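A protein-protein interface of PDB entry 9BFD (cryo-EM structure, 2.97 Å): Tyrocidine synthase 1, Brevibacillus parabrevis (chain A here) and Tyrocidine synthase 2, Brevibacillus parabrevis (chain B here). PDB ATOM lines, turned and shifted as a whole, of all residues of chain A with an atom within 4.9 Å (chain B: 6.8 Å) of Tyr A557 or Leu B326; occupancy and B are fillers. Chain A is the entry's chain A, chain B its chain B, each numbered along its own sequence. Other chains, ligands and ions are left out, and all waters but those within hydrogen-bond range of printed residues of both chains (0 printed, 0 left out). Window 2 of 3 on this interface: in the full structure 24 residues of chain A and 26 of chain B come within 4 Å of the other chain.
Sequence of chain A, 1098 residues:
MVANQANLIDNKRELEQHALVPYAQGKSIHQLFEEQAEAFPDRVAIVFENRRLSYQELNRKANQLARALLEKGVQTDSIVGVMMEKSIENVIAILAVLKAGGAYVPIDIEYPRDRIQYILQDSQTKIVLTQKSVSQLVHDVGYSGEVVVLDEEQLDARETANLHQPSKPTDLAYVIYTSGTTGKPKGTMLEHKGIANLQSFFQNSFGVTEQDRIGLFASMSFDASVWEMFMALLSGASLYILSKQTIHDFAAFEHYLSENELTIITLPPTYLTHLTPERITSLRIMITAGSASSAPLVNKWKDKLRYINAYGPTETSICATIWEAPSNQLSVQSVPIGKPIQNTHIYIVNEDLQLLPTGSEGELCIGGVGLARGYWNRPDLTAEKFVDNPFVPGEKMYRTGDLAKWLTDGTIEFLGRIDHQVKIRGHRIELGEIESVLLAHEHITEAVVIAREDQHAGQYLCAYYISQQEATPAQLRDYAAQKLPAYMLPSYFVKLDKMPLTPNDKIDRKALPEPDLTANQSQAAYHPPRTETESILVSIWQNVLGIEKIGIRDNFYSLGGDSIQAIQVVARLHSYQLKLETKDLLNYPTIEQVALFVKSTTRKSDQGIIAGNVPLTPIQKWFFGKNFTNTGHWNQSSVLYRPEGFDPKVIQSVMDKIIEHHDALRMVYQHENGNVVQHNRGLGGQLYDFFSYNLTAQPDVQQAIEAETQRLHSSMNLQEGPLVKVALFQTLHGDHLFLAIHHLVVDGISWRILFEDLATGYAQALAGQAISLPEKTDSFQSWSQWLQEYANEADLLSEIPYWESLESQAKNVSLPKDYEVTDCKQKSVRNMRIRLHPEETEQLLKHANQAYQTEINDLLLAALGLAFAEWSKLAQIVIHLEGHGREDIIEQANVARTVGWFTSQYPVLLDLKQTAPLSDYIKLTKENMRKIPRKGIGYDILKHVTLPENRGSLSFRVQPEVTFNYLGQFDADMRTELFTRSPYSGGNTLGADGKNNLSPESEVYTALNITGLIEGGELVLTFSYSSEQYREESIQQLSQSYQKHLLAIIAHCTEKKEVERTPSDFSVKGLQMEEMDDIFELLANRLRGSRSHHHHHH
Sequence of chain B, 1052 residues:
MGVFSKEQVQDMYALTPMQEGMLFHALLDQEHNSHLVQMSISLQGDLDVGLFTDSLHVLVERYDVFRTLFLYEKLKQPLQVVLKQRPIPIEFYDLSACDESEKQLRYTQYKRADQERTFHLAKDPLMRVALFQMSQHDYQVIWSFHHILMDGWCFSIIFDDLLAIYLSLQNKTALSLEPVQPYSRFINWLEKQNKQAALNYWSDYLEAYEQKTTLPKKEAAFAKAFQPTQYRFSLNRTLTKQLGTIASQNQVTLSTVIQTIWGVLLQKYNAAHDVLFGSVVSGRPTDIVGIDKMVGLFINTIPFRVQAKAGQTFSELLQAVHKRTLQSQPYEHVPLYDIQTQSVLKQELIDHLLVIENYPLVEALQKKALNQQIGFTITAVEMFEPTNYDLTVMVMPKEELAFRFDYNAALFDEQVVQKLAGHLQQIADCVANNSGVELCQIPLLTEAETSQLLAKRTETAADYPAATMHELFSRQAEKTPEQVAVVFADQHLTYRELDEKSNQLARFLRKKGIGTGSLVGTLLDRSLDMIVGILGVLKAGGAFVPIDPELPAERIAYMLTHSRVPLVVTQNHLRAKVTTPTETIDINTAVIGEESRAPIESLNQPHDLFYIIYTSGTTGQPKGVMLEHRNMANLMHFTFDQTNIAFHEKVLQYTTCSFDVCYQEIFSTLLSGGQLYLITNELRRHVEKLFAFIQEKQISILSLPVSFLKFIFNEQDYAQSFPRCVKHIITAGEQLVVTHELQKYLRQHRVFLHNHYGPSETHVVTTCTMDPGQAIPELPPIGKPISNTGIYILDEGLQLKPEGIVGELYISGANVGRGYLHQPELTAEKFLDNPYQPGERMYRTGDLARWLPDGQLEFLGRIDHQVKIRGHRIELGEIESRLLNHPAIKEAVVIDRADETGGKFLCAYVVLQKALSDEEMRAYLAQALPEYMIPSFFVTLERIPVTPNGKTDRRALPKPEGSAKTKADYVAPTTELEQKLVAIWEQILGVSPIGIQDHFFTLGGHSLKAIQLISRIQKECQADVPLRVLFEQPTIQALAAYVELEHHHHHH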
ATOM      1  N   ASN A 555      25.377  -3.251 -13.998  1.00  0.00           N
ATOM      2  CA  ASN A 555      25.204  -4.486 -14.751  1.00  0.00           C
ATOM      3  C   ASN A 555      26.560  -5.125 -15.003  1.00  0.00           C
ATOM      4  O   ASN A 555      27.497  -4.454 -15.448  1.00  0.00           O
ATOM      5  CB  ASN A 555      24.492  -4.216 -16.076  1.00  0.00           C
ATOM      6  CG  ASN A 555      24.230  -5.482 -16.862  1.00  0.00           C
ATOM      7  OD1 ASN A 555      25.154  -6.221 -17.200  1.00  0.00           O
ATOM      8  ND2 ASN A 555      22.962  -5.738 -17.160  1.00  0.00           N
ATOM      9  N   PHE A 556      26.662  -6.422 -14.702  1.00  0.00           N
ATOM     10  CA  PHE A 556      27.912  -7.146 -14.907  1.00  0.00           C
ATOM     11  C   PHE A 556      28.474  -6.915 -16.303  1.00  0.00           C
ATOM     12  O   PHE A 556      29.679  -6.687 -16.468  1.00  0.00           O
ATOM     13  CB  PHE A 556      27.689  -8.636 -14.657  1.00  0.00           C
ATOM     14  CG  PHE A 556      28.905  -9.477 -14.882  1.00  0.00           C
ATOM     15  CD1 PHE A 556      29.924  -9.501 -13.949  1.00  0.00           C
ATOM     16  CD2 PHE A 556      29.020 -10.264 -16.011  1.00  0.00           C
ATOM     17  CE1 PHE A 556      31.040 -10.278 -14.147  1.00  0.00           C
ATOM     18  CE2 PHE A 556      30.133 -11.046 -16.214  1.00  0.00           C
ATOM     19  CZ  PHE A 556      31.146 -11.052 -15.280  1.00  0.00           C
ATOM     20  N   TYR A 557      27.617  -6.972 -17.325  1.00  0.00           N
ATOM     21  CA  TYR A 557      28.072  -6.700 -18.685  1.00  0.00           C
ATOM     22  C   TYR A 557      28.372  -5.222 -18.896  1.00  0.00           C
ATOM     23  O   TYR A 557      29.383  -4.874 -19.516  1.00  0.00           O
ATOM     24  CB  TYR A 557      27.034  -7.180 -19.694  1.00  0.00           C
ATOM     25  CG  TYR A 557      26.761  -8.662 -19.653  1.00  0.00           C
ATOM     26  CD1 TYR A 557      27.699  -9.564 -20.120  1.00  0.00           C
ATOM     27  CD2 TYR A 557      25.563  -9.156 -19.173  1.00  0.00           C
ATOM     28  CE1 TYR A 557      27.460 -10.917 -20.099  1.00  0.00           C
ATOM     29  CE2 TYR A 557      25.314 -10.512 -19.150  1.00  0.00           C
ATOM     30  CZ  TYR A 557      26.268 -11.385 -19.616  1.00  0.00           C
ATOM     31  OH  TYR A 557      26.030 -12.737 -19.594  1.00  0.00           O
ATOM     32  N   SER A 558      27.518  -4.337 -18.382  1.00  0.00           N
ATOM     33  CA  SER A 558      27.761  -2.911 -18.568  1.00  0.00           C
ATOM     34  C   SER A 558      29.069  -2.480 -17.920  1.00  0.00           C
ATOM     35  O   SER A 558      29.739  -1.573 -18.423  1.00  0.00           O
ATOM     36  CB  SER A 558      26.597  -2.101 -18.006  1.00  0.00           C
ATOM     37  OG  SER A 558      26.657  -0.758 -18.446  1.00  0.00           O
ATOM     38  N   LEU A 559      29.451  -3.117 -16.813  1.00  0.00           N
ATOM     39  CA  LEU A 559      30.769  -2.885 -16.239  1.00  0.00           C
ATOM     40  C   LEU A 559      31.877  -3.521 -17.061  1.00  0.00           C
ATOM     41  O   LEU A 559      33.055  -3.269 -16.789  1.00  0.00           O
ATOM     42  CB  LEU A 559      30.826  -3.419 -14.808  1.00  0.00           C
ATOM     43  CG  LEU A 559      29.948  -2.724 -13.767  1.00  0.00           C
ATOM     44  CD1 LEU A 559      29.872  -3.560 -12.501  1.00  0.00           C
ATOM     45  CD2 LEU A 559      30.469  -1.330 -13.464  1.00  0.00           C
ATOM     46  N   GLY A 560      31.528  -4.323 -18.057  1.00  0.00           N
ATOM     47  CA  GLY A 560      32.503  -4.989 -18.886  1.00  0.00           C
ATOM     48  C   GLY A 560      32.781  -6.422 -18.497  1.00  0.00           C
ATOM     49  O   GLY A 560      33.859  -6.932 -18.818  1.00  0.00           O
ATOM     50  N   GLY A 561      31.839  -7.088 -17.839  1.00  0.00           N
ATOM     51  CA  GLY A 561      31.971  -8.495 -17.531  1.00  0.00           C
ATOM     52  C   GLY A 561      32.193  -9.312 -18.783  1.00  0.00           C
ATOM     53  O   GLY A 561      32.228  -8.762 -19.886  1.00  0.00           O
ATOM     54  N   LEU A 586      25.393 -14.782 -14.776  1.00  0.00           N
ATOM     55  CA  LEU A 586      25.188 -14.273 -16.126  1.00  0.00           C
ATOM     56  C   LEU A 586      23.724 -13.957 -16.406  1.00  0.00           C
ATOM     57  O   LEU A 586      23.429 -13.050 -17.192  1.00  0.00           O
ATOM     58  CB  LEU A 586      25.713 -15.282 -17.147  1.00  0.00           C
ATOM     59  CG  LEU A 586      27.226 -15.494 -17.160  1.00  0.00           C
ATOM     60  CD1 LEU A 586      27.587 -16.756 -17.923  1.00  0.00           C
ATOM     61  CD2 LEU A 586      27.931 -14.284 -17.754  1.00  0.00           C
ATOM     62  N   ASN A 587      22.798 -14.680 -15.778  1.00  0.00           N
ATOM     63  CA  ASN A 587      21.391 -14.590 -16.146  1.00  0.00           C
ATOM     64  C   ASN A 587      20.647 -13.513 -15.375  1.00  0.00           C
ATOM     65  O   ASN A 587      19.628 -13.011 -15.860  1.00  0.00           O
ATOM     66  CB  ASN A 587      20.703 -15.937 -15.918  1.00  0.00           C
ATOM     67  CG  ASN A 587      21.154 -16.995 -16.901  1.00  0.00           C
ATOM     68  OD1 ASN A 587      22.326 -17.060 -17.260  1.00  0.00           O
ATOM     69  ND2 ASN A 587      20.222 -17.828 -17.342  1.00  0.00           N
ATOM     70  N   PRO A 589      22.082 -10.330 -14.118  1.00  0.00           N
ATOM     71  CA  PRO A 589      23.395  -9.678 -14.095  1.00  0.00           C
ATOM     72  C   PRO A 589      23.483  -8.471 -13.179  1.00  0.00           C
ATOM     73  O   PRO A 589      24.277  -7.561 -13.434  1.00  0.00           O
ATOM     74  CB  PRO A 589      23.591  -9.278 -15.561  1.00  0.00           C
ATOM     75  CG  PRO A 589      22.207  -9.006 -16.027  1.00  0.00           C
ATOM     76  CD  PRO A 589      21.388 -10.102 -15.396  1.00  0.00           C
ATOM     77  N   TYR B 201      17.401 -30.016 -26.663  1.00  0.00           N
ATOM     78  CA  TYR B 201      17.677 -28.590 -26.782  1.00  0.00           C
ATOM     79  C   TYR B 201      18.266 -28.255 -28.135  1.00  0.00           C
ATOM     80  O   TYR B 201      17.887 -27.257 -28.757  1.00  0.00           O
ATOM     81  CB  TYR B 201      18.626 -28.110 -25.695  1.00  0.00           C
ATOM     82  CG  TYR B 201      18.923 -26.638 -25.849  1.00  0.00           C
ATOM     83  CD1 TYR B 201      18.022 -25.678 -25.423  1.00  0.00           C
ATOM     84  CD2 TYR B 201      20.093 -26.211 -26.457  1.00  0.00           C
ATOM     85  CE1 TYR B 201      18.295 -24.336 -25.566  1.00  0.00           C
ATOM     86  CE2 TYR B 201      20.368 -24.874 -26.613  1.00  0.00           C
ATOM     87  CZ  TYR B 201      19.469 -23.940 -26.166  1.00  0.00           C
ATOM     88  OH  TYR B 201      19.742 -22.605 -26.332  1.00  0.00           O
ATOM     89  N   ALA B 247      28.136  -2.219 -26.881  1.00  0.00           N
ATOM     90  CA  ALA B 247      27.962  -3.427 -26.081  1.00  0.00           C
ATOM     91  C   ALA B 247      27.569  -3.087 -24.649  1.00  0.00           C
ATOM     92  O   ALA B 247      26.612  -3.645 -24.105  1.00  0.00           O
ATOM     93  CB  ALA B 247      29.242  -4.262 -26.108  1.00  0.00           C
ATOM     94  N   SER B 248      28.306  -2.171 -24.021  1.00  0.00           N
ATOM     95  CA  SER B 248      28.034  -1.801 -22.638  1.00  0.00           C
ATOM     96  C   SER B 248      26.649  -1.200 -22.455  1.00  0.00           C
ATOM     97  O   SER B 248      26.153  -1.147 -21.325  1.00  0.00           O
ATOM     98  CB  SER B 248      29.090  -0.818 -22.137  1.00  0.00           C
ATOM     99  OG  SER B 248      28.880   0.473 -22.678  1.00  0.00           O
ATOM    100  N   GLN B 249      26.015  -0.744 -23.532  1.00  0.00           N
ATOM    101  CA  GLN B 249      24.699  -0.126 -23.418  1.00  0.00           C
ATOM    102  C   GLN B 249      23.551  -1.032 -23.841  1.00  0.00           C
ATOM    103  O   GLN B 249      22.444  -0.887 -23.312  1.00  0.00           O
ATOM    104  CB  GLN B 249      24.648   1.170 -24.233  1.00  0.00           C
ATOM    105  CG  GLN B 249      25.544   2.268 -23.687  1.00  0.00           C
ATOM    106  CD  GLN B 249      25.441   3.551 -24.479  1.00  0.00           C
ATOM    107  OE1 GLN B 249      25.001   3.551 -25.627  1.00  0.00           O
ATOM    108  NE2 GLN B 249      25.850   4.656 -23.869  1.00  0.00           N
ATOM    109  N   GLN B 251      23.647  -4.101 -23.075  1.00  0.00           N
ATOM    110  CA  GLN B 251      23.692  -5.134 -22.043  1.00  0.00           C
ATOM    111  C   GLN B 251      24.188  -6.468 -22.598  1.00  0.00           C
ATOM    112  O   GLN B 251      23.644  -7.525 -22.281  1.00  0.00           O
ATOM    113  CB  GLN B 251      22.326  -5.314 -21.378  1.00  0.00           C
ATOM    114  CG  GLN B 251      21.636  -4.024 -20.975  1.00  0.00           C
ATOM    115  CD  GLN B 251      22.451  -3.215 -19.994  1.00  0.00           C
ATOM    116  OE1 GLN B 251      23.349  -3.738 -19.338  1.00  0.00           O
ATOM    117  NE2 GLN B 251      22.136  -1.932 -19.879  1.00  0.00           N
ATOM    118  N   VAL B 252      25.225  -6.422 -23.429  1.00  0.00           N
ATOM    119  CA  VAL B 252      25.836  -7.616 -23.989  1.00  0.00           C
ATOM    120  C   VAL B 252      27.348  -7.492 -23.849  1.00  0.00           C
ATOM    121  O   VAL B 252      27.886  -6.418 -23.584  1.00  0.00           O
ATOM    122  CB  VAL B 252      25.442  -7.848 -25.462  1.00  0.00           C
ATOM    123  CG1 VAL B 252      23.949  -8.024 -25.586  1.00  0.00           C
ATOM    124  CG2 VAL B 252      25.911  -6.693 -26.320  1.00  0.00           C
ATOM    125  N   THR B 253      28.031  -8.615 -24.032  1.00  0.00           N
ATOM    126  CA  THR B 253      29.474  -8.596 -24.207  1.00  0.00           C
ATOM    127  C   THR B 253      29.842  -8.092 -25.598  1.00  0.00           C
ATOM    128  O   THR B 253      29.066  -8.204 -26.550  1.00  0.00           O
ATOM    129  CB  THR B 253      30.050  -9.991 -23.983  1.00  0.00           C
ATOM    130  OG1 THR B 253      29.406 -10.918 -24.863  1.00  0.00           O
ATOM    131  CG2 THR B 253      29.831 -10.430 -22.547  1.00  0.00           C
ATOM    132  N   VAL B 321      20.494 -12.437 -29.686  1.00  0.00           N
ATOM    133  CA  VAL B 321      21.688 -13.276 -29.679  1.00  0.00           C
ATOM    134  C   VAL B 321      22.188 -13.498 -28.259  1.00  0.00           C
ATOM    135  O   VAL B 321      22.654 -14.593 -27.915  1.00  0.00           O
ATOM    136  CB  VAL B 321      22.775 -12.645 -30.565  1.00  0.00           C
ATOM    137  CG1 VAL B 321      24.045 -13.440 -30.478  1.00  0.00           C
ATOM    138  CG2 VAL B 321      22.295 -12.563 -32.001  1.00  0.00           C
ATOM    139  N   HIS B 322      22.081 -12.482 -27.406  1.00  0.00           N
ATOM    140  CA  HIS B 322      22.452 -12.661 -26.006  1.00  0.00           C
ATOM    141  C   HIS B 322      21.601 -13.732 -25.340  1.00  0.00           C
ATOM    142  O   HIS B 322      22.123 -14.627 -24.662  1.00  0.00           O
ATOM    143  CB  HIS B 322      22.326 -11.337 -25.258  1.00  0.00           C
ATOM    144  CG  HIS B 322      22.889 -11.375 -23.875  1.00  0.00           C
ATOM    145  ND1 HIS B 322      24.114 -11.932 -23.587  1.00  0.00           N
ATOM    146  CD2 HIS B 322      22.395 -10.923 -22.699  1.00  0.00           C
ATOM    147  CE1 HIS B 322      24.351 -11.823 -22.292  1.00  0.00           C
ATOM    148  NE2 HIS B 322      23.324 -11.214 -21.730  1.00  0.00           N
ATOM    149  N   LYS B 323      20.281 -13.647 -25.506  1.00  0.00           N
ATOM    150  CA  LYS B 323      19.408 -14.654 -24.912  1.00  0.00           C
ATOM    151  C   LYS B 323      19.711 -16.047 -25.447  1.00  0.00           C
ATOM    152  O   LYS B 323      19.731 -17.022 -24.685  1.00  0.00           O
ATOM    153  CB  LYS B 323      17.945 -14.295 -25.158  1.00  0.00           C
ATOM    154  CG  LYS B 323      17.459 -13.104 -24.362  1.00  0.00           C
ATOM    155  CD  LYS B 323      16.060 -12.703 -24.782  1.00  0.00           C
ATOM    156  CE  LYS B 323      15.050 -13.770 -24.399  1.00  0.00           C
ATOM    157  NZ  LYS B 323      14.721 -13.720 -22.947  1.00  0.00           N
ATOM    158  N   ARG B 324      19.947 -16.168 -26.754  1.00  0.00           N
ATOM    159  CA  ARG B 324      20.228 -17.487 -27.315  1.00  0.00           C
ATOM    160  C   ARG B 324      21.524 -18.061 -26.763  1.00  0.00           C
ATOM    161  O   ARG B 324      21.589 -19.250 -26.421  1.00  0.00           O
ATOM    162  CB  ARG B 324      20.284 -17.424 -28.837  1.00  0.00           C
ATOM    163  CG  ARG B 324      18.960 -17.106 -29.493  1.00  0.00           C
ATOM    164  CD  ARG B 324      19.035 -17.368 -30.979  1.00  0.00           C
ATOM    165  NE  ARG B 324      18.912 -18.791 -31.262  1.00  0.00           N
ATOM    166  CZ  ARG B 324      17.764 -19.409 -31.495  1.00  0.00           C
ATOM    167  NH1 ARG B 324      16.623 -18.744 -31.562  1.00  0.00           N
ATOM    168  NH2 ARG B 324      17.763 -20.725 -31.688  1.00  0.00           N
ATOM    169  N   THR B 325      22.564 -17.235 -26.651  1.00  0.00           N
ATOM    170  CA  THR B 325      23.829 -17.737 -26.124  1.00  0.00           C
ATOM    171  C   THR B 325      23.712 -18.109 -24.653  1.00  0.00           C
ATOM    172  O   THR B 325      24.320 -19.088 -24.207  1.00  0.00           O
ATOM    173  CB  THR B 325      24.938 -16.706 -26.335  1.00  0.00           C
ATOM    174  OG1 THR B 325      26.208 -17.305 -26.049  1.00  0.00           O
ATOM    175  CG2 THR B 325      24.741 -15.509 -25.425  1.00  0.00           C
ATOM    176  N   LEU B 326      22.945 -17.341 -23.877  1.00  0.00           N
ATOM    177  CA  LEU B 326      22.694 -17.729 -22.493  1.00  0.00           C
ATOM    178  C   LEU B 326      21.945 -19.053 -22.401  1.00  0.00           C
ATOM    179  O   LEU B 326      22.259 -19.894 -21.552  1.00  0.00           O
ATOM    180  CB  LEU B 326      21.921 -16.630 -21.769  1.00  0.00           C
ATOM    181  CG  LEU B 326      22.699 -15.361 -21.448  1.00  0.00           C
ATOM    182  CD1 LEU B 326      21.820 -14.394 -20.691  1.00  0.00           C
ATOM    183  CD2 LEU B 326      23.925 -15.707 -20.637  1.00  0.00           C
ATOM    184  N   GLN B 327      20.949 -19.258 -23.264  1.00  0.00           N
ATOM    185  CA  GLN B 327      20.215 -20.518 -23.249  1.00  0.00           C
ATOM    186  C   GLN B 327      21.069 -21.697 -23.691  1.00  0.00           C
ATOM    187  O   GLN B 327      20.832 -22.827 -23.251  1.00  0.00           O
ATOM    188  CB  GLN B 327      18.981 -20.415 -24.142  1.00  0.00           C
ATOM    189  CG  GLN B 327      17.888 -19.531 -23.588  1.00  0.00           C
ATOM    190  CD  GLN B 327      16.766 -19.322 -24.576  1.00  0.00           C
ATOM    191  OE1 GLN B 327      16.728 -19.956 -25.629  1.00  0.00           O
ATOM    192  NE2 GLN B 327      15.848 -18.423 -24.246  1.00  0.00           N
ATOM    193  N   SER B 328      22.056 -21.465 -24.551  1.00  0.00           N
ATOM    194  CA  SER B 328      22.849 -22.578 -25.060  1.00  0.00           C
ATOM    195  C   SER B 328      23.875 -23.077 -24.048  1.00  0.00           C
ATOM    196  O   SER B 328      24.248 -24.252 -24.081  1.00  0.00           O
ATOM    197  CB  SER B 328      23.544 -22.166 -26.356  1.00  0.00           C
ATOM    198  OG  SER B 328      24.365 -23.210 -26.847  1.00  0.00           O
ATOM    199  N   GLN B 329      24.338 -22.208 -23.157  1.00  0.00           N
ATOM    200  CA  GLN B 329      25.434 -22.555 -22.257  1.00  0.00           C
ATOM    201  C   GLN B 329      25.232 -23.831 -21.451  1.00  0.00           C
ATOM    202  O   GLN B 329      26.218 -24.560 -21.249  1.00  0.00           O
ATOM    203  CB  GLN B 329      25.689 -21.380 -21.305  1.00  0.00           C
ATOM    204  CG  GLN B 329      26.893 -21.562 -20.403  1.00  0.00           C
ATOM    205  CD  GLN B 329      27.348 -20.258 -19.780  1.00  0.00           C
ATOM    206  OE1 GLN B 329      26.860 -19.184 -20.133  1.00  0.00           O
ATOM    207  NE2 GLN B 329      28.289 -20.345 -18.846  1.00  0.00           N
ATOM    208  N   PRO B 330      24.034 -24.164 -20.965  1.00  0.00           N
ATOM    209  CA  PRO B 330      23.863 -25.465 -20.298  1.00  0.00           C
ATOM    210  C   PRO B 330      24.175 -26.671 -21.166  1.00  0.00           C
ATOM    211  O   PRO B 330      24.538 -27.724 -20.629  1.00  0.00           O
ATOM    212  CB  PRO B 330      22.387 -25.442 -19.881  1.00  0.00           C
ATOM    213  CG  PRO B 330      22.060 -24.002 -19.768  1.00  0.00           C
ATOM    214  CD  PRO B 330      22.817 -23.343 -20.876  1.00  0.00           C
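Among the printed residues, merely in contact across the chains: Tyr A557 with His B322, Tyr A557 with Thr B253, Leu A586 with Gln B329, Tyr A557 with Leu B326, Ser A558 with Gln B251, Leu A586 with Leu B326, Gly A561 with Thr B253 and Asn A587 with Leu B326.
Printed residues of chain B within 4 Å of Tyr A557: Thr B253 (3.3 Å), His B322 (3.3 Å) and Leu B326 (3.8 Å). Of the printed residues of chain B, Leu A586 touches Leu B326 and Gln B329. Of the printed residues of chain A, Ser B248 touches Ser A558 (2.9 Å). Of chain A, only Tyr A557 (3.8 Å), Leu A586 (3.9 Å) and Asn A587 (3.97 Å) come within 4 Å of Leu B326. Of the printed residues of chain A, Gln B329 touches Leu A586 (3.4 Å). The nearest printed residue of chain B that does not touch Tyr A557 is Gln B251 (4.0003 Å). The nearest printed residue of chain A that does not touch Leu B326 is Pro A589 (6.8 Å). The nearest printed residue of chain B that does not touch Gly A561 is Val B252 (6.2 Å).
N of Gly A561 is in hydrogen-bond range of O of Phe A556 (2.6 Å). The side-chain amide oxygen (OD1) of Asn A555 lies within hydrogen-bond range of the backbone NH (N) of Tyr A557 (2.6 Å). The side-chain amide oxygen of Asn A555 is in hydrogen-bond range of the backbone NH of Ser A558.
Hydrophobic or aromatic side chains of chain B within 4 Å of the printed part of chain A: His B322 and Leu B326. Hydrophobic or aromatic side chains of chain A that line the printed part of chain B: Tyr A557 and Leu A586. Among the printed residues, 10 pairs touch across the chains. Among the printed residues, no Asp or Glu carboxylate lies within 4 Å of a Lys or Arg side-chain nitrogen of the other chain.
The side-chain hydroxyl (OG) of Ser A558 is in hydrogen-bond range of the backbone carbonyl oxygen (O) of Ser B248 (2.9 Å). The side-chain amide nitrogen of Asn A555 is in hydrogen-bond range of the side-chain amide oxygen of Gln B251 (3.0 Å).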
